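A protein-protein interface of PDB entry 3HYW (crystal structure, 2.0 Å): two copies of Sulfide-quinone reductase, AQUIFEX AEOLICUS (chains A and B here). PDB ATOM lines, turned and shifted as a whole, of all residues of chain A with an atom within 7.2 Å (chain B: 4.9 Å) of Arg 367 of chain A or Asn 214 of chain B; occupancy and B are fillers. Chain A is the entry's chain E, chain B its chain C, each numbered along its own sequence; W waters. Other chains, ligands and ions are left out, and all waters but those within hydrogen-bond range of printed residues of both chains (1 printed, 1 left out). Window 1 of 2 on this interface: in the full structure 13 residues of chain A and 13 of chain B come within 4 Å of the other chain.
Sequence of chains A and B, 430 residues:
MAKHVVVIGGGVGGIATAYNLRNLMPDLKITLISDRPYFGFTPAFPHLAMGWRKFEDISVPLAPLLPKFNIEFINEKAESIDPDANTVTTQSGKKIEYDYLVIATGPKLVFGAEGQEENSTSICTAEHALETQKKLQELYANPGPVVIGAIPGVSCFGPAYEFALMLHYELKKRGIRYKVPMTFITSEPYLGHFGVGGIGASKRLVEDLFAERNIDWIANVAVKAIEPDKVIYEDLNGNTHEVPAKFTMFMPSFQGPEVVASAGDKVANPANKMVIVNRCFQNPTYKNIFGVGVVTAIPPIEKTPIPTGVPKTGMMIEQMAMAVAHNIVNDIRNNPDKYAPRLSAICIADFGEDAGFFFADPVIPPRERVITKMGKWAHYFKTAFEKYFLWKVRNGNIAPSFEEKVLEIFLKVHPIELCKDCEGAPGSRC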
ATOM      1  N   HIS A 193     -13.457  28.085   7.654  1.00  0.00           N
ATOM      2  CA  HIS A 193     -12.958  27.140   6.655  1.00  0.00           C
ATOM      3  C   HIS A 193     -12.926  25.729   7.265  1.00  0.00           C
ATOM      4  O   HIS A 193     -13.331  24.755   6.618  1.00  0.00           O
ATOM      5  CB  HIS A 193     -11.569  27.572   6.161  1.00  0.00           C
ATOM      6  CG  HIS A 193     -10.989  26.682   5.100  1.00  0.00           C
ATOM      7  ND1 HIS A 193     -10.322  25.510   5.391  1.00  0.00           N
ATOM      8  CD2 HIS A 193     -10.968  26.799   3.751  1.00  0.00           C
ATOM      9  CE1 HIS A 193      -9.919  24.941   4.270  1.00  0.00           C
ATOM     10  NE2 HIS A 193     -10.293  25.705   3.260  1.00  0.00           N
ATOM     11  N   GLY A 195     -10.874  23.554   7.671  1.00  0.00           N
ATOM     12  CA  GLY A 195     -10.102  22.541   6.967  1.00  0.00           C
ATOM     13  C   GLY A 195     -10.961  21.729   6.019  1.00  0.00           C
ATOM     14  O   GLY A 195     -10.553  20.657   5.585  1.00  0.00           O
ATOM     15  N   VAL A 196     -12.153  22.237   5.701  1.00  0.00           N
ATOM     16  CA  VAL A 196     -13.114  21.506   4.854  1.00  0.00           C
ATOM     17  C   VAL A 196     -13.643  22.341   3.693  1.00  0.00           C
ATOM     18  O   VAL A 196     -14.578  21.933   2.992  1.00  0.00           O
ATOM     19  CB  VAL A 196     -14.308  20.903   5.679  1.00  0.00           C
ATOM     20  CG1 VAL A 196     -13.804  19.917   6.709  1.00  0.00           C
ATOM     21  CG2 VAL A 196     -15.144  22.002   6.356  1.00  0.00           C
ATOM     22  N   GLY A 197     -13.031  23.502   3.477  1.00  0.00           N
ATOM     23  CA  GLY A 197     -13.502  24.437   2.466  1.00  0.00           C
ATOM     24  C   GLY A 197     -14.779  25.121   2.905  1.00  0.00           C
ATOM     25  O   GLY A 197     -15.518  25.657   2.083  1.00  0.00           O
ATOM     26  N   GLY A 198     -15.034  25.105   4.209  1.00  0.00           N
ATOM     27  CA  GLY A 198     -16.233  25.703   4.776  1.00  0.00           C
ATOM     28  C   GLY A 198     -17.428  24.770   4.753  1.00  0.00           C
ATOM     29  O   GLY A 198     -17.457  23.796   3.993  1.00  0.00           O
ATOM     30  N   ILE A 199     -18.413  25.070   5.595  1.00  0.00           N
ATOM     31  CA  ILE A 199     -19.658  24.304   5.636  1.00  0.00           C
ATOM     32  C   ILE A 199     -20.820  25.261   5.422  1.00  0.00           C
ATOM     33  O   ILE A 199     -21.147  26.064   6.298  1.00  0.00           O
ATOM     34  CB  ILE A 199     -19.839  23.519   6.975  1.00  0.00           C
ATOM     35  CG1 ILE A 199     -18.712  22.498   7.165  1.00  0.00           C
ATOM     36  CG2 ILE A 199     -21.215  22.825   7.019  1.00  0.00           C
ATOM     37  CD1 ILE A 199     -18.650  21.865   8.568  1.00  0.00           C
ATOM     38  N   GLY A 200     -21.441  25.172   4.252  1.00  0.00           N
ATOM     39  CA  GLY A 200     -22.480  26.114   3.868  1.00  0.00           C
ATOM     40  C   GLY A 200     -21.965  27.528   4.043  1.00  0.00           C
ATOM     41  O   GLY A 200     -20.835  27.829   3.668  1.00  0.00           O
ATOM     42  N   ILE A 301      -8.592  18.479   1.923  1.00  0.00           N
ATOM     43  CA  ILE A 301      -9.685  18.760   0.993  1.00  0.00           C
ATOM     44  C   ILE A 301      -9.207  19.787  -0.022  1.00  0.00           C
ATOM     45  O   ILE A 301      -9.380  19.609  -1.228  1.00  0.00           O
ATOM     46  CB  ILE A 301     -10.980  19.196   1.747  1.00  0.00           C
ATOM     47  CG1 ILE A 301     -11.638  17.958   2.375  1.00  0.00           C
ATOM     48  CG2 ILE A 301     -11.940  19.937   0.809  1.00  0.00           C
ATOM     49  CD1 ILE A 301     -12.684  18.234   3.442  1.00  0.00           C
ATOM     50  N   ARG A 342     -19.363   6.672   5.252  1.00  0.00           N
ATOM     51  CA  ARG A 342     -19.902   7.826   4.548  1.00  0.00           C
ATOM     52  C   ARG A 342     -19.074   9.080   4.835  1.00  0.00           C
ATOM     53  O   ARG A 342     -18.946   9.946   3.977  1.00  0.00           O
ATOM     54  CB  ARG A 342     -21.372   8.044   4.931  1.00  0.00           C
ATOM     55  CG  ARG A 342     -22.023   9.293   4.336  1.00  0.00           C
ATOM     56  CD  ARG A 342     -22.391   9.121   2.866  1.00  0.00           C
ATOM     57  NE  ARG A 342     -23.124  10.288   2.386  1.00  0.00           N
ATOM     58  CZ  ARG A 342     -23.741  10.379   1.211  1.00  0.00           C
ATOM     59  NH1 ARG A 342     -23.738   9.357   0.361  1.00  0.00           N
ATOM     60  NH2 ARG A 342     -24.379  11.498   0.898  1.00  0.00           N
ATOM     61  N   PHE A 359     -23.798  20.558  10.007  1.00  0.00           N
ATOM     62  CA  PHE A 359     -23.943  19.214   9.458  1.00  0.00           C
ATOM     63  C   PHE A 359     -23.417  19.238   8.029  1.00  0.00           C
ATOM     64  O   PHE A 359     -23.801  20.100   7.243  1.00  0.00           O
ATOM     65  CB  PHE A 359     -25.406  18.758   9.512  1.00  0.00           C
ATOM     66  CG  PHE A 359     -25.678  17.450   8.796  1.00  0.00           C
ATOM     67  CD1 PHE A 359     -26.511  17.415   7.690  1.00  0.00           C
ATOM     68  CD2 PHE A 359     -25.104  16.258   9.237  1.00  0.00           C
ATOM     69  CE1 PHE A 359     -26.770  16.219   7.027  1.00  0.00           C
ATOM     70  CE2 PHE A 359     -25.352  15.056   8.579  1.00  0.00           C
ATOM     71  CZ  PHE A 359     -26.187  15.039   7.475  1.00  0.00           C
ATOM     72  N   ALA A 360     -22.508  18.319   7.712  1.00  0.00           N
ATOM     73  CA  ALA A 360     -21.980  18.182   6.355  1.00  0.00           C
ATOM     74  C   ALA A 360     -22.026  16.715   5.945  1.00  0.00           C
ATOM     75  O   ALA A 360     -21.472  15.861   6.639  1.00  0.00           O
ATOM     76  CB  ALA A 360     -20.566  18.713   6.276  1.00  0.00           C
ATOM     77  N   ASP A 361     -22.697  16.432   4.832  1.00  0.00           N
ATOM     78  CA  ASP A 361     -22.819  15.068   4.323  1.00  0.00           C
ATOM     79  C   ASP A 361     -22.457  14.956   2.841  1.00  0.00           C
ATOM     80  O   ASP A 361     -23.216  15.414   1.983  1.00  0.00           O
ATOM     81  CB  ASP A 361     -24.242  14.538   4.536  1.00  0.00           C
ATOM     82  CG  ASP A 361     -24.421  13.102   4.030  1.00  0.00           C
ATOM     83  OD1 ASP A 361     -23.475  12.299   4.161  1.00  0.00           O
ATOM     84  OD2 ASP A 361     -25.508  12.780   3.499  1.00  0.00           O
ATOM     85  N   PRO A 362     -21.286  14.363   2.533  1.00  0.00           N
ATOM     86  CA  PRO A 362     -20.174  14.037   3.435  1.00  0.00           C
ATOM     87  C   PRO A 362     -19.360  15.274   3.816  1.00  0.00           C
ATOM     88  O   PRO A 362     -19.574  16.354   3.263  1.00  0.00           O
ATOM     89  CB  PRO A 362     -19.302  13.093   2.593  1.00  0.00           C
ATOM     90  CG  PRO A 362     -20.131  12.715   1.409  1.00  0.00           C
ATOM     91  CD  PRO A 362     -21.029  13.874   1.169  1.00  0.00           C
ATOM     92  N   VAL A 363     -18.436  15.115   4.756  1.00  0.00           N
ATOM     93  CA  VAL A 363     -17.518  16.197   5.127  1.00  0.00           C
ATOM     94  C   VAL A 363     -16.594  16.532   3.953  1.00  0.00           C
ATOM     95  O   VAL A 363     -16.401  17.703   3.625  1.00  0.00           O
ATOM     96  CB  VAL A 363     -16.697  15.854   6.389  1.00  0.00           C
ATOM     97  CG1 VAL A 363     -15.684  16.941   6.687  1.00  0.00           C
ATOM     98  CG2 VAL A 363     -17.619  15.686   7.579  1.00  0.00           C
ATOM     99  N   ILE A 364     -16.037  15.503   3.325  1.00  0.00           N
ATOM    100  CA  ILE A 364     -15.235  15.690   2.124  1.00  0.00           C
ATOM    101  C   ILE A 364     -16.163  15.874   0.916  1.00  0.00           C
ATOM    102  O   ILE A 364     -16.961  14.977   0.600  1.00  0.00           O
ATOM    103  CB  ILE A 364     -14.227  14.516   1.897  1.00  0.00           C
ATOM    104  CG1 ILE A 364     -13.288  14.374   3.107  1.00  0.00           C
ATOM    105  CG2 ILE A 364     -13.423  14.732   0.613  1.00  0.00           C
ATOM    106  CD1 ILE A 364     -12.686  12.985   3.285  1.00  0.00           C
ATOM    107  N   PRO A 365     -16.074  17.047   0.248  1.00  0.00           N
ATOM    108  CA  PRO A 365     -16.869  17.382  -0.926  1.00  0.00           C
ATOM    109  C   PRO A 365     -16.636  16.439  -2.114  1.00  0.00           C
ATOM    110  O   PRO A 365     -15.624  15.733  -2.145  1.00  0.00           O
ATOM    111  CB  PRO A 365     -16.393  18.801  -1.270  1.00  0.00           C
ATOM    112  CG  PRO A 365     -15.840  19.334  -0.023  1.00  0.00           C
ATOM    113  CD  PRO A 365     -15.193  18.168   0.629  1.00  0.00           C
ATOM    114  N   PRO A 366     -17.564  16.427  -3.094  1.00  0.00           N
ATOM    115  CA  PRO A 366     -18.812  17.200  -3.114  1.00  0.00           C
ATOM    116  C   PRO A 366     -19.859  16.674  -2.131  1.00  0.00           C
ATOM    117  O   PRO A 366     -19.918  15.478  -1.850  1.00  0.00           O
ATOM    118  CB  PRO A 366     -19.299  17.053  -4.555  1.00  0.00           C
ATOM    119  CG  PRO A 366     -18.705  15.775  -5.028  1.00  0.00           C
ATOM    120  CD  PRO A 366     -17.393  15.625  -4.321  1.00  0.00           C
ATOM    121  N   ARG A 367     -20.680  17.585  -1.628  1.00  0.00           N
ATOM    122  CA  ARG A 367     -21.637  17.281  -0.582  1.00  0.00           C
ATOM    123  C   ARG A 367     -23.043  17.082  -1.129  1.00  0.00           C
ATOM    124  O   ARG A 367     -23.448  17.738  -2.090  1.00  0.00           O
ATOM    125  CB  ARG A 367     -21.634  18.398   0.461  1.00  0.00           C
ATOM    126  CG  ARG A 367     -20.237  18.787   0.929  1.00  0.00           C
ATOM    127  CD  ARG A 367     -20.260  19.259   2.354  1.00  0.00           C
ATOM    128  NE  ARG A 367     -18.915  19.401   2.903  1.00  0.00           N
ATOM    129  CZ  ARG A 367     -18.293  20.562   3.070  1.00  0.00           C
ATOM    130  NH1 ARG A 367     -17.073  20.585   3.585  1.00  0.00           N
ATOM    131  NH2 ARG A 367     -18.884  21.695   2.725  1.00  0.00           N
ATOM    132  N   GLU A 368     -23.776  16.169  -0.502  1.00  0.00           N
ATOM    133  CA  GLU A 368     -25.187  15.951  -0.785  1.00  0.00           C
ATOM    134  C   GLU A 368     -25.995  17.081  -0.159  1.00  0.00           C
ATOM    135  O   GLU A 368     -26.857  17.659  -0.809  1.00  0.00           O
ATOM    136  CB  GLU A 368     -25.635  14.596  -0.219  1.00  0.00           C
ATOM    137  CG  GLU A 368     -26.889  14.009  -0.862  1.00  0.00           C
ATOM    138  CD  GLU A 368     -26.649  13.445  -2.261  1.00  0.00           C
ATOM    139  OE1 GLU A 368     -25.501  13.067  -2.582  1.00  0.00           O
ATOM    140  OE2 GLU A 368     -27.623  13.373  -3.043  1.00  0.00           O
ATOM    141  N   ARG A 369     -25.714  17.389   1.107  1.00  0.00           N
ATOM    142  CA  ARG A 369     -26.364  18.517   1.780  1.00  0.00           C
ATOM    143  C   ARG A 369     -25.553  19.008   2.977  1.00  0.00           C
ATOM    144  O   ARG A 369     -24.697  18.292   3.490  1.00  0.00           O
ATOM    145  CB  ARG A 369     -27.805  18.163   2.200  1.00  0.00           C
ATOM    146  CG  ARG A 369     -27.921  17.288   3.450  1.00  0.00           C
ATOM    147  CD  ARG A 369     -29.327  16.701   3.592  1.00  0.00           C
ATOM    148  NE  ARG A 369     -29.474  15.482   2.790  1.00  0.00           N
ATOM    149  CZ  ARG A 369     -30.274  15.350   1.736  1.00  0.00           C
ATOM    150  NH1 ARG A 369     -31.042  16.355   1.343  1.00  0.00           N
ATOM    151  NH2 ARG A 369     -30.322  14.199   1.079  1.00  0.00           N
ATOM    152  N   VAL A 370     -25.816  20.246   3.385  1.00  0.00           N
ATOM    153  CA  VAL A 370     -25.286  20.798   4.628  1.00  0.00           C
ATOM    154  C   VAL A 370     -26.419  21.456   5.415  1.00  0.00           C
ATOM    155  O   VAL A 370     -27.446  21.826   4.847  1.00  0.00           O
ATOM    156  CB  VAL A 370     -24.146  21.846   4.402  1.00  0.00           C
ATOM    157  CG1 VAL A 370     -22.932  21.220   3.729  1.00  0.00           C
ATOM    158  CG2 VAL A 370     -24.647  23.066   3.616  1.00  0.00           C
ATOM    159  N   ARG A 429     -14.532   8.473  -3.711  1.00  0.00           N
ATOM    160  CA  ARG A 429     -15.744   7.710  -3.985  1.00  0.00           C
ATOM    161  C   ARG A 429     -15.470   6.454  -4.801  1.00  0.00           C
ATOM    162  O   ARG A 429     -14.765   6.514  -5.813  1.00  0.00           O
ATOM    163  CB  ARG A 429     -16.778   8.596  -4.690  1.00  0.00           C
ATOM    164  CG  ARG A 429     -17.675   9.416  -3.757  1.00  0.00           C
ATOM    165  CD  ARG A 429     -16.901  10.361  -2.840  1.00  0.00           C
ATOM    166  NE  ARG A 429     -17.646  11.594  -2.606  1.00  0.00           N
ATOM    167  CZ  ARG A 429     -17.390  12.477  -1.648  1.00  0.00           C
ATOM    168  NH1 ARG A 429     -16.396  12.287  -0.787  1.00  0.00           N
ATOM    169  NH2 ARG A 429     -18.146  13.561  -1.551  1.00  0.00           N
ATOM    170  N   ARG B 177     -25.302  13.284  -6.107  1.00  0.00           N
ATOM    171  CA  ARG B 177     -24.695  14.617  -5.980  1.00  0.00           C
ATOM    172  C   ARG B 177     -23.318  14.559  -5.297  1.00  0.00           C
ATOM    173  O   ARG B 177     -22.401  15.301  -5.659  1.00  0.00           O
ATOM    174  CB  ARG B 177     -25.669  15.555  -5.238  1.00  0.00           C
ATOM    175  CG  ARG B 177     -25.268  17.031  -5.068  1.00  0.00           C
ATOM    176  CD  ARG B 177     -24.924  17.751  -6.370  1.00  0.00           C
ATOM    177  NE  ARG B 177     -23.489  17.985  -6.440  1.00  0.00           N
ATOM    178  CZ  ARG B 177     -22.872  19.091  -6.034  1.00  0.00           C
ATOM    179  NH1 ARG B 177     -23.555  20.111  -5.540  1.00  0.00           N
ATOM    180  NH2 ARG B 177     -21.557  19.174  -6.128  1.00  0.00           N
ATOM    181  N   TYR B 178     -23.170  13.645  -4.338  1.00  0.00           N
ATOM    182  CA  TYR B 178     -21.910  13.469  -3.614  1.00  0.00           C
ATOM    183  C   TYR B 178     -20.810  12.821  -4.463  1.00  0.00           C
ATOM    184  O   TYR B 178     -19.660  12.729  -4.030  1.00  0.00           O
ATOM    185  CB  TYR B 178     -22.134  12.685  -2.310  1.00  0.00           C
ATOM    186  CG  TYR B 178     -22.212  11.184  -2.467  1.00  0.00           C
ATOM    187  CD1 TYR B 178     -21.201  10.360  -1.961  1.00  0.00           C
ATOM    188  CD2 TYR B 178     -23.293  10.581  -3.111  1.00  0.00           C
ATOM    189  CE1 TYR B 178     -21.266   8.974  -2.090  1.00  0.00           C
ATOM    190  CE2 TYR B 178     -23.367   9.192  -3.244  1.00  0.00           C
ATOM    191  CZ  TYR B 178     -22.350   8.400  -2.739  1.00  0.00           C
ATOM    192  OH  TYR B 178     -22.422   7.032  -2.869  1.00  0.00           O
ATOM    193  N   MET B 182     -19.293  20.146  -8.572  1.00  0.00           N
ATOM    194  CA  MET B 182     -19.885  21.197  -9.383  1.00  0.00           C
ATOM    195  C   MET B 182     -19.153  22.506  -9.181  1.00  0.00           C
ATOM    196  O   MET B 182     -18.931  22.940  -8.052  1.00  0.00           O
ATOM    197  CB  MET B 182     -21.373  21.371  -9.074  1.00  0.00           C
ATOM    198  CG  MET B 182     -22.225  20.212  -9.556  1.00  0.00           C
ATOM    199  SD  MET B 182     -23.986  20.479  -9.333  1.00  0.00           S
ATOM    200  CE  MET B 182     -24.304  21.591 -10.712  1.00  0.00           C
ATOM    201  N   PHE B 210     -25.218  29.124  -3.525  1.00  0.00           N
ATOM    202  CA  PHE B 210     -24.130  28.242  -3.937  1.00  0.00           C
ATOM    203  C   PHE B 210     -23.416  27.589  -2.747  1.00  0.00           C
ATOM    204  O   PHE B 210     -23.095  26.399  -2.789  1.00  0.00           O
ATOM    205  CB  PHE B 210     -23.133  29.016  -4.809  1.00  0.00           C
ATOM    206  CG  PHE B 210     -23.539  29.132  -6.260  1.00  0.00           C
ATOM    207  CD1 PHE B 210     -24.852  28.917  -6.666  1.00  0.00           C
ATOM    208  CD2 PHE B 210     -22.598  29.482  -7.218  1.00  0.00           C
ATOM    209  CE1 PHE B 210     -25.214  29.032  -8.016  1.00  0.00           C
ATOM    210  CE2 PHE B 210     -22.953  29.608  -8.558  1.00  0.00           C
ATOM    211  CZ  PHE B 210     -24.260  29.386  -8.955  1.00  0.00           C
ATOM    212  N   ALA B 211     -23.174  28.363  -1.689  1.00  0.00           N
ATOM    213  CA  ALA B 211     -22.565  27.827  -0.467  1.00  0.00           C
ATOM    214  C   ALA B 211     -23.410  26.704   0.144  1.00  0.00           C
ATOM    215  O   ALA B 211     -22.883  25.655   0.541  1.00  0.00           O
ATOM    216  CB  ALA B 211     -22.330  28.937   0.553  1.00  0.00           C
ATOM    217  N   GLU B 212     -24.720  26.931   0.202  1.00  0.00           N
ATOM    218  CA  GLU B 212     -25.668  25.957   0.749  1.00  0.00           C
ATOM    219  C   GLU B 212     -25.788  24.698  -0.103  1.00  0.00           C
ATOM    220  O   GLU B 212     -26.081  23.624   0.414  1.00  0.00           O
ATOM    221  CB  GLU B 212     -27.050  26.597   0.907  1.00  0.00           C
ATOM    222  CG  GLU B 212     -27.155  27.544   2.098  1.00  0.00           C
ATOM    223  CD  GLU B 212     -28.444  28.350   2.114  1.00  0.00           C
ATOM    224  OE1 GLU B 212     -28.993  28.654   1.024  1.00  0.00           O
ATOM    225  OE2 GLU B 212     -28.906  28.686   3.228  1.00  0.00           O
ATOM    226  N   ARG B 213     -25.573  24.835  -1.407  1.00  0.00           N
ATOM    227  CA  ARG B 213     -25.734  23.713  -2.334  1.00  0.00           C
ATOM    228  C   ARG B 213     -24.394  23.142  -2.825  1.00  0.00           C
ATOM    229  O   ARG B 213     -24.358  22.331  -3.754  1.00  0.00           O
ATOM    230  CB  ARG B 213     -26.704  24.094  -3.470  1.00  0.00           C
ATOM    231  CG  ARG B 213     -28.139  24.202  -2.953  1.00  0.00           C
ATOM    232  CD  ARG B 213     -29.180  24.829  -3.897  1.00  0.00           C
ATOM    233  NE  ARG B 213     -30.251  25.397  -3.075  1.00  0.00           N
ATOM    234  CZ  ARG B 213     -31.519  25.593  -3.440  1.00  0.00           C
ATOM    235  NH1 ARG B 213     -31.950  25.275  -4.652  1.00  0.00           N
ATOM    236  NH2 ARG B 213     -32.374  26.111  -2.564  1.00  0.00           N
ATOM    237  N   ASN B 214     -23.311  23.547  -2.154  1.00  0.00           N
ATOM    238  CA  ASN B 214     -21.929  23.134  -2.467  1.00  0.00           C
ATOM    239  C   ASN B 214     -21.584  23.259  -3.951  1.00  0.00           C
ATOM    240  O   ASN B 214     -20.997  22.359  -4.555  1.00  0.00           O
ATOM    241  CB  ASN B 214     -21.620  21.723  -1.919  1.00  0.00           C
ATOM    242  CG  ASN B 214     -20.153  21.312  -2.100  1.00  0.00           C
ATOM    243  OD1 ASN B 214     -19.222  22.080  -1.832  1.00  0.00           O
ATOM    244  ND2 ASN B 214     -19.949  20.092  -2.551  1.00  0.00           N
ATOM    245  N   ILE B 215     -21.976  24.385  -4.539  1.00  0.00           N
ATOM    246  CA  ILE B 215     -21.545  24.710  -5.887  1.00  0.00           C
ATOM    247  C   ILE B 215     -20.334  25.633  -5.761  1.00  0.00           C
ATOM    248  O   ILE B 215     -20.455  26.789  -5.338  1.00  0.00           O
ATOM    249  CB  ILE B 215     -22.692  25.319  -6.738  1.00  0.00           C
ATOM    250  CG1 ILE B 215     -23.792  24.263  -6.951  1.00  0.00           C
ATOM    251  CG2 ILE B 215     -22.168  25.817  -8.083  1.00  0.00           C
ATOM    252  CD1 ILE B 215     -25.133  24.820  -7.351  1.00  0.00           C
ATOM    253  N   ASP B 216     -19.159  25.102  -6.088  1.00  0.00           N
ATOM    254  CA  ASP B 216     -17.939  25.909  -6.088  1.00  0.00           C
ATOM    255  C   ASP B 216     -18.052  26.950  -7.190  1.00  0.00           C
ATOM    256  O   ASP B 216     -18.736  26.719  -8.181  1.00  0.00           O
ATOM    257  CB  ASP B 216     -16.709  25.038  -6.321  1.00  0.00           C
ATOM    258  CG  ASP B 216     -16.487  24.024  -5.212  1.00  0.00           C
ATOM    259  OD1 ASP B 216     -16.705  24.347  -4.021  1.00  0.00           O
ATOM    260  OD2 ASP B 216     -16.079  22.892  -5.542  1.00  0.00           O
HETATM  261  O   HOH W   1     -27.736  21.590   1.307  1.00  0.00           O
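Of the 22 printed residues of chain A, 9 touch a printed residue of chain B.
Hydrophobic or aromatic side chains of chain A that line the printed part of chain B: Pro 362, Pro 365, Pro 366 and Val 370.
Along chain B the printed residues that touch a printed residue of chain A span positions 177 to 214.
Among the printed residues, no Asp or Glu carboxylate lies within 4 Å of a Lys or Arg side-chain nitrogen of the other chain.
The side-chain carboxylate (OE1) of Glu 368 of chain A is in hydrogen-bond range of the backbone NH (N) of Tyr 178 of chain B.
The guanidinium group (NE) of Arg 429 of chain A is in hydrogen-bond range of the backbone carbonyl oxygen (O) of Tyr 178 of chain B (2.7 Å).
The side-chain amide nitrogen (ND2) of Asn 214 of chain B sits close to the backbone NH (N) of Arg 367 of chain A (2.8 Å).
The backbone carbonyl oxygen (O) of Gly 198 of chain A is in hydrogen-bond range of the guanidinium group (NH2) of Arg 367 of chain A (2.8 Å).
The guanidinium group of Arg 342 of chain A is in salt-bridge range of the side-chain carboxylate of Asp 361 of chain A (2.7 Å).
The guanidinium group of Arg 342 of chain A is in salt-bridge range of the side-chain carboxylate of Glu 368 of chain A (3.98 Å).
The backbone NH of Glu 368 of chain A lies within hydrogen-bond range of the backbone carbonyl oxygen of Asp 361 of chain A (2.7 Å).
The backbone carbonyl oxygen (O) of Ile 364 of chain A lies within hydrogen-bond range of the guanidinium group (NH2) of Arg 429 of chain A (2.8 Å).
The backbone carbonyl oxygen (O) of Pro 366 of chain A sits at hydrogen-bond distance from the guanidinium group (NH2) of Arg 429 of chain A (2.6 Å).
Water W1 bridges O of Glu 212 of chain B (2.8 Å) and N of Val 370 of chain A (3.1 Å).
Of the printed residues of chain B, Arg 367 of chain A touches Arg 177 and Asn 214.
Printed residues of chain A within 4 Å of Asn 214 of chain B: Pro 365, Pro 366 and Arg 367.
Printed residues of chain B within 4 Å of Pro 362 of chain A: Tyr 178 (3.8 Å).
Printed residues of chain A within 4 Å of Glu 212 of chain B: Val 370.
Of the printed residues of chain B, Arg 342 of chain A touches Tyr 178.
Printed residues of chain A within 4 Å of Tyr 178 of chain B: Arg 342, Pro 362, Pro 366, Glu 368 and Arg 429.
Of the printed residues of chain B, Gly 200 of chain A touches Ala 211.
Met 182 of chain B touches none of the printed residues of chain A.
The nearest printed residue of chain B that does not touch Pro 366 of chain A is Met 182 of chain B (5.1 Å).
Among the printed residues, merely in contact across the chains: Pro 366 of chain A with Asn 214 of chain B, Pro 366 of chain A with Tyr 178 of chain B, Gly 200 of chain A with Ala 211 of chain B, Pro 366 of chain A with Arg 177 of chain B, Arg 342 of chain A with Tyr 178 of chain B, Glu 368 of chain A with Arg 177 of chain B, Val 370 of chain A with Glu 212 of chain B, Arg 367 of chain A with Arg 177 of chain B, Pro 362 of chain A with Tyr 178 of chain B and Pro 365 of chain A with Asn 214 of chain B.
No position is printed for both chains.
Of the 13 pairs that touch across the chains among the printed residues, none has its exchanged pair printed and touching as well.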
